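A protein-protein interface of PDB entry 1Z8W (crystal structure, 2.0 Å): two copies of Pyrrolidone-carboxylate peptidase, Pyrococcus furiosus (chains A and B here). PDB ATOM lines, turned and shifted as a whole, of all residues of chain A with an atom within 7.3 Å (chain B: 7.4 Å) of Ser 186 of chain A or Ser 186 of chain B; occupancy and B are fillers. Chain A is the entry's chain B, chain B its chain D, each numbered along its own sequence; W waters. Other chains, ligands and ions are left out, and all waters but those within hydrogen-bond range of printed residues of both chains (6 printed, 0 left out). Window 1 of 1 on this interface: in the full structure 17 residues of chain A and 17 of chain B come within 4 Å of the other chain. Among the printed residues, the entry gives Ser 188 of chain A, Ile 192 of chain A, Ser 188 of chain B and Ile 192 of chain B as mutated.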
ATOM      1  N   GLY A  72     -25.357   9.324  -8.984  1.00  0.00           N
ATOM      2  CA  GLY A  72     -24.238   9.644  -9.848  1.00  0.00           C
ATOM      3  C   GLY A  72     -23.422  10.860  -9.462  1.00  0.00           C
ATOM      4  O   GLY A  72     -22.244  10.948  -9.817  1.00  0.00           O
ATOM      5  N   ARG A  73     -24.021  11.809  -8.754  1.00  0.00           N
ATOM      6  CA  ARG A  73     -23.262  12.982  -8.358  1.00  0.00           C
ATOM      7  C   ARG A  73     -22.278  12.627  -7.242  1.00  0.00           C
ATOM      8  O   ARG A  73     -22.575  11.822  -6.357  1.00  0.00           O
ATOM      9  CB  ARG A  73     -24.216  14.130  -8.003  1.00  0.00           C
ATOM     10  CG  ARG A  73     -24.605  14.876  -9.284  1.00  0.00           C
ATOM     11  CD  ARG A  73     -26.067  15.239  -9.434  1.00  0.00           C
ATOM     12  NE  ARG A  73     -26.364  16.547  -8.881  1.00  0.00           N
ATOM     13  CZ  ARG A  73     -27.205  17.429  -9.418  1.00  0.00           C
ATOM     14  NH1 ARG A  73     -27.851  17.162 -10.547  1.00  0.00           N
ATOM     15  NH2 ARG A  73     -27.418  18.578  -8.802  1.00  0.00           N
ATOM     16  N   SER A  74     -21.088  13.212  -7.324  1.00  0.00           N
ATOM     17  CA  SER A  74     -19.999  12.927  -6.392  1.00  0.00           C
ATOM     18  C   SER A  74     -19.858  13.822  -5.172  1.00  0.00           C
ATOM     19  O   SER A  74     -19.025  13.555  -4.304  1.00  0.00           O
ATOM     20  CB  SER A  74     -18.684  12.960  -7.156  1.00  0.00           C
ATOM     21  OG  SER A  74     -18.489  14.257  -7.689  1.00  0.00           O
ATOM     22  N   ALA A  75     -20.646  14.883  -5.101  1.00  0.00           N
ATOM     23  CA  ALA A  75     -20.551  15.786  -3.967  1.00  0.00           C
ATOM     24  C   ALA A  75     -21.889  16.453  -3.725  1.00  0.00           C
ATOM     25  O   ALA A  75     -22.826  16.284  -4.505  1.00  0.00           O
ATOM     26  CB  ALA A  75     -19.486  16.843  -4.236  1.00  0.00           C
ATOM     27  N   PRO A 130     -17.070  18.426   0.228  1.00  0.00           N
ATOM     28  CA  PRO A 130     -17.134  18.814  -1.182  1.00  0.00           C
ATOM     29  C   PRO A 130     -18.551  19.223  -1.575  1.00  0.00           C
ATOM     30  O   PRO A 130     -19.521  18.517  -1.283  1.00  0.00           O
ATOM     31  CB  PRO A 130     -16.638  17.567  -1.918  1.00  0.00           C
ATOM     32  CG  PRO A 130     -16.894  16.454  -0.966  1.00  0.00           C
ATOM     33  CD  PRO A 130     -16.573  17.051   0.380  1.00  0.00           C
ATOM     34  N   PRO A 168     -25.357  12.787  -2.923  1.00  0.00           N
ATOM     35  CA  PRO A 168     -24.924  11.571  -3.617  1.00  0.00           C
ATOM     36  C   PRO A 168     -25.513  10.343  -2.931  1.00  0.00           C
ATOM     37  O   PRO A 168     -26.136  10.449  -1.871  1.00  0.00           O
ATOM     38  CB  PRO A 168     -23.404  11.590  -3.450  1.00  0.00           C
ATOM     39  CG  PRO A 168     -23.076  13.043  -3.166  1.00  0.00           C
ATOM     40  CD  PRO A 168     -24.215  13.472  -2.293  1.00  0.00           C
ATOM     41  N   TYR A 169     -25.312   9.182  -3.543  1.00  0.00           N
ATOM     42  CA  TYR A 169     -25.747   7.923  -2.948  1.00  0.00           C
ATOM     43  C   TYR A 169     -24.882   7.791  -1.695  1.00  0.00           C
ATOM     44  O   TYR A 169     -23.801   8.382  -1.628  1.00  0.00           O
ATOM     45  CB  TYR A 169     -25.343   6.731  -3.821  1.00  0.00           C
ATOM     46  CG  TYR A 169     -26.174   6.409  -5.037  1.00  0.00           C
ATOM     47  CD1 TYR A 169     -27.513   6.044  -4.918  1.00  0.00           C
ATOM     48  CD2 TYR A 169     -25.585   6.356  -6.300  1.00  0.00           C
ATOM     49  CE1 TYR A 169     -28.242   5.617  -6.031  1.00  0.00           C
ATOM     50  CE2 TYR A 169     -26.301   5.933  -7.411  1.00  0.00           C
ATOM     51  CZ  TYR A 169     -27.624   5.561  -7.271  1.00  0.00           C
ATOM     52  OH  TYR A 169     -28.318   5.106  -8.368  1.00  0.00           O
ATOM     53  N   ILE A 170     -25.338   7.024  -0.707  1.00  0.00           N
ATOM     54  CA  ILE A 170     -24.489   6.769   0.445  1.00  0.00           C
ATOM     55  C   ILE A 170     -23.846   5.429   0.055  1.00  0.00           C
ATOM     56  O   ILE A 170     -24.405   4.679  -0.750  1.00  0.00           O
ATOM     57  CB  ILE A 170     -25.275   6.661   1.784  1.00  0.00           C
ATOM     58  CG1 ILE A 170     -26.434   5.679   1.661  1.00  0.00           C
ATOM     59  CG2 ILE A 170     -25.768   8.040   2.204  1.00  0.00           C
ATOM     60  CD1 ILE A 170     -27.136   5.444   2.992  1.00  0.00           C
ATOM     61  N   PRO A 171     -22.665   5.115   0.606  1.00  0.00           N
ATOM     62  CA  PRO A 171     -21.938   3.875   0.301  1.00  0.00           C
ATOM     63  C   PRO A 171     -22.718   2.563   0.202  1.00  0.00           C
ATOM     64  O   PRO A 171     -22.523   1.793  -0.742  1.00  0.00           O
ATOM     65  CB  PRO A 171     -20.867   3.832   1.388  1.00  0.00           C
ATOM     66  CG  PRO A 171     -20.570   5.287   1.610  1.00  0.00           C
ATOM     67  CD  PRO A 171     -21.964   5.884   1.649  1.00  0.00           C
ATOM     68  N   GLU A 172     -23.592   2.292   1.165  1.00  0.00           N
ATOM     69  CA  GLU A 172     -24.336   1.038   1.137  1.00  0.00           C
ATOM     70  C   GLU A 172     -25.192   0.857  -0.106  1.00  0.00           C
ATOM     71  O   GLU A 172     -25.517  -0.270  -0.473  1.00  0.00           O
ATOM     72  CB  GLU A 172     -25.202   0.903   2.389  1.00  0.00           C
ATOM     73  CG  GLU A 172     -26.135   2.061   2.639  1.00  0.00           C
ATOM     74  CD  GLU A 172     -26.719   2.018   4.035  1.00  0.00           C
ATOM     75  OE1 GLU A 172     -27.767   1.361   4.223  1.00  0.00           O
ATOM     76  OE2 GLU A 172     -26.112   2.630   4.944  1.00  0.00           O
ATOM     77  N   GLN A 173     -25.547   1.959  -0.758  1.00  0.00           N
ATOM     78  CA  GLN A 173     -26.377   1.902  -1.958  1.00  0.00           C
ATOM     79  C   GLN A 173     -25.583   1.493  -3.190  1.00  0.00           C
ATOM     80  O   GLN A 173     -26.156   1.141  -4.220  1.00  0.00           O
ATOM     81  CB  GLN A 173     -27.025   3.265  -2.223  1.00  0.00           C
ATOM     82  CG  GLN A 173     -28.067   3.672  -1.210  1.00  0.00           C
ATOM     83  CD  GLN A 173     -28.711   4.998  -1.559  1.00  0.00           C
ATOM     84  OE1 GLN A 173     -28.091   6.054  -1.432  1.00  0.00           O
ATOM     85  NE2 GLN A 173     -29.961   4.948  -2.017  1.00  0.00           N
ATOM     86  N   ILE A 174     -24.261   1.553  -3.083  1.00  0.00           N
ATOM     87  CA  ILE A 174     -23.384   1.204  -4.191  1.00  0.00           C
ATOM     88  C   ILE A 174     -23.155  -0.302  -4.346  1.00  0.00           C
ATOM     89  O   ILE A 174     -22.921  -0.789  -5.455  1.00  0.00           O
ATOM     90  CB  ILE A 174     -21.998   1.883  -4.028  1.00  0.00           C
ATOM     91  CG1 ILE A 174     -22.165   3.393  -3.830  1.00  0.00           C
ATOM     92  CG2 ILE A 174     -21.133   1.602  -5.246  1.00  0.00           C
ATOM     93  CD1 ILE A 174     -22.918   4.083  -4.948  1.00  0.00           C
ATOM     94  N   VAL A 183     -19.616   1.572 -10.943  1.00  0.00           N
ATOM     95  CA  VAL A 183     -19.456   2.018  -9.568  1.00  0.00           C
ATOM     96  C   VAL A 183     -19.624   3.524  -9.413  1.00  0.00           C
ATOM     97  O   VAL A 183     -18.659   4.286  -9.517  1.00  0.00           O
ATOM     98  CB  VAL A 183     -18.076   1.610  -9.016  1.00  0.00           C
ATOM     99  CG1 VAL A 183     -18.054   1.780  -7.508  1.00  0.00           C
ATOM    100  CG2 VAL A 183     -17.767   0.173  -9.405  1.00  0.00           C
ATOM    101  N   PRO A 184     -20.863   3.978  -9.173  1.00  0.00           N
ATOM    102  CA  PRO A 184     -21.091   5.416  -9.009  1.00  0.00           C
ATOM    103  C   PRO A 184     -20.477   5.943  -7.710  1.00  0.00           C
ATOM    104  O   PRO A 184     -20.181   5.173  -6.791  1.00  0.00           O
ATOM    105  CB  PRO A 184     -22.615   5.536  -9.037  1.00  0.00           C
ATOM    106  CG  PRO A 184     -23.080   4.213  -8.522  1.00  0.00           C
ATOM    107  CD  PRO A 184     -22.135   3.233  -9.170  1.00  0.00           C
ATOM    108  N   PRO A 185     -20.267   7.265  -7.630  1.00  0.00           N
ATOM    109  CA  PRO A 185     -19.688   7.913  -6.449  1.00  0.00           C
ATOM    110  C   PRO A 185     -20.651   7.835  -5.269  1.00  0.00           C
ATOM    111  O   PRO A 185     -21.854   7.622  -5.452  1.00  0.00           O
ATOM    112  CB  PRO A 185     -19.494   9.363  -6.901  1.00  0.00           C
ATOM    113  CG  PRO A 185     -19.479   9.286  -8.398  1.00  0.00           C
ATOM    114  CD  PRO A 185     -20.518   8.249  -8.695  1.00  0.00           C
ATOM    115  N   SER A 186     -20.119   8.013  -4.063  1.00  0.00           N
ATOM    116  CA  SER A 186     -20.935   7.994  -2.860  1.00  0.00           C
ATOM    117  C   SER A 186     -20.329   8.920  -1.807  1.00  0.00           C
ATOM    118  O   SER A 186     -19.181   9.356  -1.930  1.00  0.00           O
ATOM    119  CB  SER A 186     -21.064   6.565  -2.309  1.00  0.00           C
ATOM    120  OG  SER A 186     -19.804   5.996  -1.986  1.00  0.00           O
ATOM    121  N   MET A 187     -21.119   9.229  -0.785  1.00  0.00           N
ATOM    122  CA  MET A 187     -20.691  10.099   0.303  1.00  0.00           C
ATOM    123  C   MET A 187     -21.332   9.567   1.578  1.00  0.00           C
ATOM    124  O   MET A 187     -22.493   9.159   1.563  1.00  0.00           O
ATOM    125  CB  MET A 187     -21.142  11.541   0.040  1.00  0.00           C
ATOM    126  CG  MET A 187     -20.705  12.528   1.119  1.00  0.00           C
ATOM    127  SD  MET A 187     -21.075  14.228   0.682  1.00  0.00           S
ATOM    128  CE  MET A 187     -19.669  14.636  -0.378  1.00  0.00           C
ATOM    129  N   SER A 188     -20.584   9.566   2.676  1.00  0.00           N
ATOM    130  CA  SER A 188     -21.112   9.040   3.933  1.00  0.00           C
ATOM    131  C   SER A 188     -22.390   9.744   4.361  1.00  0.00           C
ATOM    132  O   SER A 188     -22.573  10.934   4.110  1.00  0.00           O
ATOM    133  CB  SER A 188     -20.073   9.162   5.053  1.00  0.00           C
ATOM    134  OG  SER A 188     -19.982  10.498   5.525  1.00  0.00           O
ATOM    135  N   MET A 191     -21.705  12.721   6.637  1.00  0.00           N
ATOM    136  CA  MET A 191     -21.282  13.958   5.985  1.00  0.00           C
ATOM    137  C   MET A 191     -22.461  14.678   5.348  1.00  0.00           C
ATOM    138  O   MET A 191     -22.571  15.900   5.433  1.00  0.00           O
ATOM    139  CB  MET A 191     -20.217  13.683   4.922  1.00  0.00           C
ATOM    140  CG  MET A 191     -19.772  14.942   4.184  1.00  0.00           C
ATOM    141  SD  MET A 191     -18.267  14.700   3.230  1.00  0.00           S
ATOM    142  CE  MET A 191     -17.035  14.896   4.509  1.00  0.00           C
ATOM    143  N   ILE A 192     -23.338  13.917   4.699  1.00  0.00           N
ATOM    144  CA  ILE A 192     -24.510  14.500   4.063  1.00  0.00           C
ATOM    145  C   ILE A 192     -25.409  15.152   5.103  1.00  0.00           C
ATOM    146  O   ILE A 192     -25.916  16.256   4.893  1.00  0.00           O
ATOM    147  CB  ILE A 192     -25.318  13.431   3.301  1.00  0.00           C
ATOM    148  CG1 ILE A 192     -24.495  12.904   2.123  1.00  0.00           C
ATOM    149  CG2 ILE A 192     -26.623  14.024   2.811  1.00  0.00           C
ATOM    150  CD1 ILE A 192     -25.091  11.676   1.454  1.00  0.00           C
ATOM    151  N   GLY B  72      -9.676   9.692  -8.633  1.00  0.00           N
ATOM    152  CA  GLY B  72     -10.775   9.470  -9.555  1.00  0.00           C
ATOM    153  C   GLY B  72     -11.598   8.218  -9.322  1.00  0.00           C
ATOM    154  O   GLY B  72     -12.756   8.153  -9.731  1.00  0.00           O
ATOM    155  N   ARG B  73     -11.018   7.205  -8.688  1.00  0.00           N
ATOM    156  CA  ARG B  73     -11.793   6.001  -8.431  1.00  0.00           C
ATOM    157  C   ARG B  73     -12.798   6.257  -7.312  1.00  0.00           C
ATOM    158  O   ARG B  73     -12.508   6.974  -6.356  1.00  0.00           O
ATOM    159  CB  ARG B  73     -10.851   4.821  -8.164  1.00  0.00           C
ATOM    160  CG  ARG B  73     -10.439   4.209  -9.503  1.00  0.00           C
ATOM    161  CD  ARG B  73      -8.978   3.849  -9.647  1.00  0.00           C
ATOM    162  NE  ARG B  73      -8.705   2.487  -9.223  1.00  0.00           N
ATOM    163  CZ  ARG B  73      -7.847   1.664  -9.821  1.00  0.00           C
ATOM    164  NH1 ARG B  73      -7.167   2.049 -10.890  1.00  0.00           N
ATOM    165  NH2 ARG B  73      -7.650   0.453  -9.329  1.00  0.00           N
ATOM    166  N   SER B  74     -13.990   5.685  -7.468  1.00  0.00           N
ATOM    167  CA  SER B  74     -15.104   5.892  -6.542  1.00  0.00           C
ATOM    168  C   SER B  74     -15.277   4.888  -5.417  1.00  0.00           C
ATOM    169  O   SER B  74     -16.118   5.081  -4.541  1.00  0.00           O
ATOM    170  CB  SER B  74     -16.408   5.937  -7.338  1.00  0.00           C
ATOM    171  OG  SER B  74     -16.599   4.694  -7.999  1.00  0.00           O
ATOM    172  N   ALA B  75     -14.504   3.811  -5.436  1.00  0.00           N
ATOM    173  CA  ALA B  75     -14.627   2.806  -4.395  1.00  0.00           C
ATOM    174  C   ALA B  75     -13.300   2.112  -4.185  1.00  0.00           C
ATOM    175  O   ALA B  75     -12.348   2.342  -4.930  1.00  0.00           O
ATOM    176  CB  ALA B  75     -15.688   1.779  -4.785  1.00  0.00           C
ATOM    177  N   PRO B 130     -18.234  -0.216  -0.571  1.00  0.00           N
ATOM    178  CA  PRO B 130     -18.131  -0.466  -2.013  1.00  0.00           C
ATOM    179  C   PRO B 130     -16.703  -0.840  -2.401  1.00  0.00           C
ATOM    180  O   PRO B 130     -15.740  -0.176  -2.009  1.00  0.00           O
ATOM    181  CB  PRO B 130     -18.608   0.850  -2.640  1.00  0.00           C
ATOM    182  CG  PRO B 130     -18.396   1.863  -1.571  1.00  0.00           C
ATOM    183  CD  PRO B 130     -18.744   1.136  -0.299  1.00  0.00           C
ATOM    184  N   PRO B 168      -9.842   5.659  -2.949  1.00  0.00           N
ATOM    185  CA  PRO B 168     -10.252   6.940  -3.531  1.00  0.00           C
ATOM    186  C   PRO B 168      -9.673   8.090  -2.717  1.00  0.00           C
ATOM    187  O   PRO B 168      -9.069   7.875  -1.665  1.00  0.00           O
ATOM    188  CB  PRO B 168     -11.778   6.916  -3.406  1.00  0.00           C
ATOM    189  CG  PRO B 168     -12.121   5.445  -3.282  1.00  0.00           C
ATOM    190  CD  PRO B 168     -11.005   4.919  -2.423  1.00  0.00           C
ATOM    191  N   TYR B 169      -9.861   9.308  -3.210  1.00  0.00           N
ATOM    192  CA  TYR B 169      -9.436  10.501  -2.485  1.00  0.00           C
ATOM    193  C   TYR B 169     -10.336  10.519  -1.258  1.00  0.00           C
ATOM    194  O   TYR B 169     -11.425   9.946  -1.293  1.00  0.00           O
ATOM    195  CB  TYR B 169      -9.808  11.776  -3.246  1.00  0.00           C
ATOM    196  CG  TYR B 169      -8.948  12.198  -4.401  1.00  0.00           C
ATOM    197  CD1 TYR B 169      -7.609  12.548  -4.214  1.00  0.00           C
ATOM    198  CD2 TYR B 169      -9.508  12.378  -5.667  1.00  0.00           C
ATOM    199  CE1 TYR B 169      -6.854  13.077  -5.260  1.00  0.00           C
ATOM    200  CE2 TYR B 169      -8.763  12.906  -6.715  1.00  0.00           C
ATOM    201  CZ  TYR B 169      -7.443  13.258  -6.503  1.00  0.00           C
ATOM    202  OH  TYR B 169      -6.728  13.821  -7.534  1.00  0.00           O
ATOM    203  N   ILE B 170      -9.906  11.178  -0.186  1.00  0.00           N
ATOM    204  CA  ILE B 170     -10.783  11.322   0.969  1.00  0.00           C
ATOM    205  C   ILE B 170     -11.411  12.696   0.701  1.00  0.00           C
ATOM    206  O   ILE B 170     -10.829  13.519  -0.017  1.00  0.00           O
ATOM    207  CB  ILE B 170     -10.033  11.294   2.332  1.00  0.00           C
ATOM    208  CG1 ILE B 170      -8.869  12.278   2.336  1.00  0.00           C
ATOM    209  CG2 ILE B 170      -9.569   9.870   2.629  1.00  0.00           C
ATOM    210  CD1 ILE B 170      -8.192  12.388   3.701  1.00  0.00           C
ATOM    211  N   PRO B 171     -12.604  12.958   1.251  1.00  0.00           N
ATOM    212  CA  PRO B 171     -13.317  14.228   1.055  1.00  0.00           C
ATOM    213  C   PRO B 171     -12.532  15.539   1.104  1.00  0.00           C
ATOM    214  O   PRO B 171     -12.695  16.387   0.222  1.00  0.00           O
ATOM    215  CB  PRO B 171     -14.415  14.169   2.112  1.00  0.00           C
ATOM    216  CG  PRO B 171     -14.722  12.698   2.167  1.00  0.00           C
ATOM    217  CD  PRO B 171     -13.332  12.099   2.200  1.00  0.00           C
ATOM    218  N   GLU B 172     -11.692  15.722   2.117  1.00  0.00           N
ATOM    219  CA  GLU B 172     -10.936  16.969   2.227  1.00  0.00           C
ATOM    220  C   GLU B 172     -10.042  17.260   1.027  1.00  0.00           C
ATOM    221  O   GLU B 172      -9.697  18.414   0.769  1.00  0.00           O
ATOM    222  CB  GLU B 172     -10.097  16.977   3.512  1.00  0.00           C
ATOM    223  CG  GLU B 172      -9.182  15.788   3.675  1.00  0.00           C
ATOM    224  CD  GLU B 172      -8.629  15.692   5.078  1.00  0.00           C
ATOM    225  OE1 GLU B 172      -7.585  16.322   5.345  1.00  0.00           O
ATOM    226  OE2 GLU B 172      -9.252  15.000   5.917  1.00  0.00           O
ATOM    227  N   GLN B 173      -9.675  16.221   0.284  1.00  0.00           N
ATOM    228  CA  GLN B 173      -8.813  16.390  -0.882  1.00  0.00           C
ATOM    229  C   GLN B 173      -9.572  16.926  -2.087  1.00  0.00           C
ATOM    230  O   GLN B 173      -8.968  17.386  -3.056  1.00  0.00           O
ATOM    231  CB  GLN B 173      -8.169  15.058  -1.266  1.00  0.00           C
ATOM    232  CG  GLN B 173      -7.155  14.539  -0.275  1.00  0.00           C
ATOM    233  CD  GLN B 173      -6.514  13.253  -0.747  1.00  0.00           C
ATOM    234  OE1 GLN B 173      -7.146  12.194  -0.744  1.00  0.00           O
ATOM    235  NE2 GLN B 173      -5.254  13.340  -1.172  1.00  0.00           N
ATOM    236  N   ILE B 174     -10.896  16.857  -2.024  1.00  0.00           N
ATOM    237  CA  ILE B 174     -11.745  17.318  -3.113  1.00  0.00           C
ATOM    238  C   ILE B 174     -11.969  18.831  -3.126  1.00  0.00           C
ATOM    239  O   ILE B 174     -12.179  19.418  -4.187  1.00  0.00           O
ATOM    240  CB  ILE B 174     -13.134  16.634  -3.046  1.00  0.00           C
ATOM    241  CG1 ILE B 174     -12.970  15.110  -2.983  1.00  0.00           C
ATOM    242  CG2 ILE B 174     -13.974  17.040  -4.247  1.00  0.00           C
ATOM    243  CD1 ILE B 174     -12.212  14.518  -4.153  1.00  0.00           C
ATOM    244  N   VAL B 183     -15.345  17.637  -9.970  1.00  0.00           N
ATOM    245  CA  VAL B 183     -15.539  17.056  -8.651  1.00  0.00           C
ATOM    246  C   VAL B 183     -15.380  15.541  -8.647  1.00  0.00           C
ATOM    247  O   VAL B 183     -16.341  14.799  -8.860  1.00  0.00           O
ATOM    248  CB  VAL B 183     -16.929  17.421  -8.087  1.00  0.00           C
ATOM    249  CG1 VAL B 183     -16.981  17.110  -6.599  1.00  0.00           C
ATOM    250  CG2 VAL B 183     -17.221  18.895  -8.338  1.00  0.00           C
ATOM    251  N   PRO B 184     -14.150  15.060  -8.413  1.00  0.00           N
ATOM    252  CA  PRO B 184     -13.931  13.613  -8.386  1.00  0.00           C
ATOM    253  C   PRO B 184     -14.583  12.969  -7.158  1.00  0.00           C
ATOM    254  O   PRO B 184     -14.902  13.650  -6.183  1.00  0.00           O
ATOM    255  CB  PRO B 184     -12.404  13.489  -8.380  1.00  0.00           C
ATOM    256  CG  PRO B 184     -11.955  14.754  -7.710  1.00  0.00           C
ATOM    257  CD  PRO B 184     -12.880  15.798  -8.296  1.00  0.00           C
ATOM    258  N   PRO B 185     -14.803  11.645  -7.209  1.00  0.00           N
ATOM    259  CA  PRO B 185     -15.415  10.883  -6.117  1.00  0.00           C
ATOM    260  C   PRO B 185     -14.482  10.836  -4.917  1.00  0.00           C
ATOM    261  O   PRO B 185     -13.274  11.051  -5.052  1.00  0.00           O
ATOM    262  CB  PRO B 185     -15.601   9.487  -6.718  1.00  0.00           C
ATOM    263  CG  PRO B 185     -15.562   9.707  -8.198  1.00  0.00           C
ATOM    264  CD  PRO B 185     -14.507  10.763  -8.349  1.00  0.00           C
ATOM    265  N   SER B 186     -15.043  10.551  -3.749  1.00  0.00           N
ATOM    266  CA  SER B 186     -14.256  10.448  -2.530  1.00  0.00           C
ATOM    267  C   SER B 186     -14.886   9.422  -1.590  1.00  0.00           C
ATOM    268  O   SER B 186     -16.023   9.000  -1.793  1.00  0.00           O
ATOM    269  CB  SER B 186     -14.142  11.820  -1.840  1.00  0.00           C
ATOM    270  OG  SER B 186     -15.412  12.360  -1.515  1.00  0.00           O
ATOM    271  N   MET B 187     -14.129   9.009  -0.581  1.00  0.00           N
ATOM    272  CA  MET B 187     -14.596   8.040   0.405  1.00  0.00           C
ATOM    273  C   MET B 187     -13.986   8.450   1.740  1.00  0.00           C
ATOM    274  O   MET B 187     -12.826   8.858   1.789  1.00  0.00           O
ATOM    275  CB  MET B 187     -14.137   6.627   0.020  1.00  0.00           C
ATOM    276  CG  MET B 187     -14.592   5.534   0.982  1.00  0.00           C
ATOM    277  SD  MET B 187     -14.209   3.882   0.373  1.00  0.00           S
ATOM    278  CE  MET B 187     -15.601   3.586  -0.716  1.00  0.00           C
ATOM    279  N   SER B 188     -14.759   8.350   2.818  1.00  0.00           N
ATOM    280  CA  SER B 188     -14.258   8.749   4.133  1.00  0.00           C
ATOM    281  C   SER B 188     -12.991   8.001   4.514  1.00  0.00           C
ATOM    282  O   SER B 188     -12.807   6.842   4.140  1.00  0.00           O
ATOM    283  CB  SER B 188     -15.323   8.516   5.211  1.00  0.00           C
ATOM    284  OG  SER B 188     -15.409   7.143   5.547  1.00  0.00           O
ATOM    285  N   MET B 191     -13.746   4.807   6.477  1.00  0.00           N
ATOM    286  CA  MET B 191     -14.153   3.638   5.705  1.00  0.00           C
ATOM    287  C   MET B 191     -12.955   2.984   5.024  1.00  0.00           C
ATOM    288  O   MET B 191     -12.854   1.754   4.977  1.00  0.00           O
ATOM    289  CB  MET B 191     -15.200   4.013   4.653  1.00  0.00           C
ATOM    290  CG  MET B 191     -15.612   2.845   3.764  1.00  0.00           C
ATOM    291  SD  MET B 191     -17.090   3.169   2.761  1.00  0.00           S
ATOM    292  CE  MET B 191     -18.381   2.893   3.998  1.00  0.00           C
ATOM    293  N   ILE B 192     -12.059   3.805   4.485  1.00  0.00           N
ATOM    294  CA  ILE B 192     -10.871   3.288   3.817  1.00  0.00           C
ATOM    295  C   ILE B 192      -9.996   2.523   4.805  1.00  0.00           C
ATOM    296  O   ILE B 192      -9.490   1.448   4.491  1.00  0.00           O
ATOM    297  CB  ILE B 192     -10.048   4.420   3.190  1.00  0.00           C
ATOM    298  CG1 ILE B 192     -10.840   5.059   2.044  1.00  0.00           C
ATOM    299  CG2 ILE B 192      -8.729   3.873   2.667  1.00  0.00           C
ATOM    300  CD1 ILE B 192     -10.225   6.341   1.517  1.00  0.00           C
HETATM  301  O   HOH W   1     -16.260  13.813  -3.889  1.00  0.00           O
HETATM  302  O   HOH W   2     -18.929   4.711  -4.257  1.00  0.00           O
HETATM  303  O   HOH W   3     -17.206   7.674  -4.137  1.00  0.00           O
HETATM  304  O   HOH W   4     -18.078  10.841  -3.996  1.00  0.00           O
HETATM  305  O   HOH W   5     -17.511  11.185  -0.480  1.00  0.00           O
HETATM  306  O   HOH W   6     -17.593   6.964  -0.585  1.00  0.00           O
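Of the printed residues of chain A, Ser 74 of chain B touches Val 183, Pro 184 and Pro 185. Of the printed residues of chain A, Ile 174 of chain B touches Pro 130 (3.6 Å). Printed residues of chain A within 4 Å of Pro 184 of chain B: Ser 74 (3.9 Å). Of the printed residues of chain A, Pro 185 of chain B touches Pro 185. Ser 186 of chain B touches just one residue of chain A: Ser 186. The nearest residue of chain B that does not touch Ser 186 of chain A is Pro 130 of chain B (4.4 Å). The nearest residue of chain A that does not touch Ser 186 of chain B is Pro 130 of chain A (4.4 Å).
OG of Ser 188 of chain B lies within hydrogen-bond range of N of Met 191 of chain B, 3.0 Å away. OG of Ser 188 of chain A lies within hydrogen-bond range of N of Met 191 of chain A.
Water W1 lies within hydrogen-bond range of O of Pro 184 of chain B, O of Ser 74 of chain A and OG of Ser 186 of chain B. Water W6 lies within hydrogen-bond range of OG of Ser 186 of chain A and O of Ser 186 of chain B. Water W3 lies within hydrogen-bond range of the backbone carbonyl oxygen of Ser 74 of chain B (2.8 Å), the backbone NH of Ser 186 of chain A (2.9 Å) and the backbone carbonyl oxygen of Ser 186 of chain B (2.9 Å).
Pro 130 of chain A touches Ile 174 of chain B, and with the chains exchanged Ile 174 of chain A touches Pro 130 of chain B. Pro 185 of chain B touches its own counterpart, Pro 185 of chain A. Ser 186 of chain A touches its own counterpart, Ser 186 of chain B. Positions printed for both chains: 72, 73, 74, 75, 130, 168, 169, 170, 171, 172, 173, 174, 183, 184, 185, 186, 187, 188, 191 and 192. Of the 15 pairs that touch across the chains among the printed residues, 14 have their exchanged pair printed and touching as well.
Printed residues of chain B that touch a printed residue of chain A: Ser 74, Ala 75, Pro 130, Pro 171, Ile 174, Val 183, Pro 184, Pro 185, Ser 186 and Met 191. Hydrophobic or aromatic side chains of chain B within 4 Å of the printed part of chain A: Ala 75, Pro 130, Pro 171, Ile 174, Val 183, Pro 185 and Met 191. Of the 20 printed residues of chain A, 10 touch a printed residue of chain B. Along chain A the printed residues that touch a printed residue of chain B span positions 74 to 191. Among the printed residues, 15 pairs touch across the chains.
Pro 184 of chain B touches Ser 74 of chain A (O to OG, 3.9 Å). Ala 75 of chain A touches Val 183 of chain B. Pro 130 of chain A touches Pro 171 of chain B. Ile 174 of chain B touches Pro 130 of chain A (CG2 to CB, 3.6 Å). Pro 171 of chain A touches Pro 130 of chain B (CB to CD, 3.8 Å). Pro 171 of chain A touches Met 191 of chain B (CB to CE, 3.7 Å). Val 183 of chain A touches Ala 75 of chain B (CG1 to CB, 3.6 Å). OG of Ser 74 of chain B touches O of Pro 184 of chain A, 3.8 Å away. Pro 185 of chain A touches Pro 185 of chain B (CB to CB, 3.9 Å).
The side-chain hydroxyl (OG) of Ser 74 of chain B lies within hydrogen-bond range of the backbone carbonyl oxygen (O) of Val 183 of chain A (2.6 Å). OG of Ser 74 of chain A is in hydrogen-bond range of O of Val 183 of chain B, at 2.5 Å. The backbone carbonyl oxygen of Ser 186 of chain A sits close to the backbone carbonyl oxygen of Ser 186 of chain B, 3.2 Å away.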
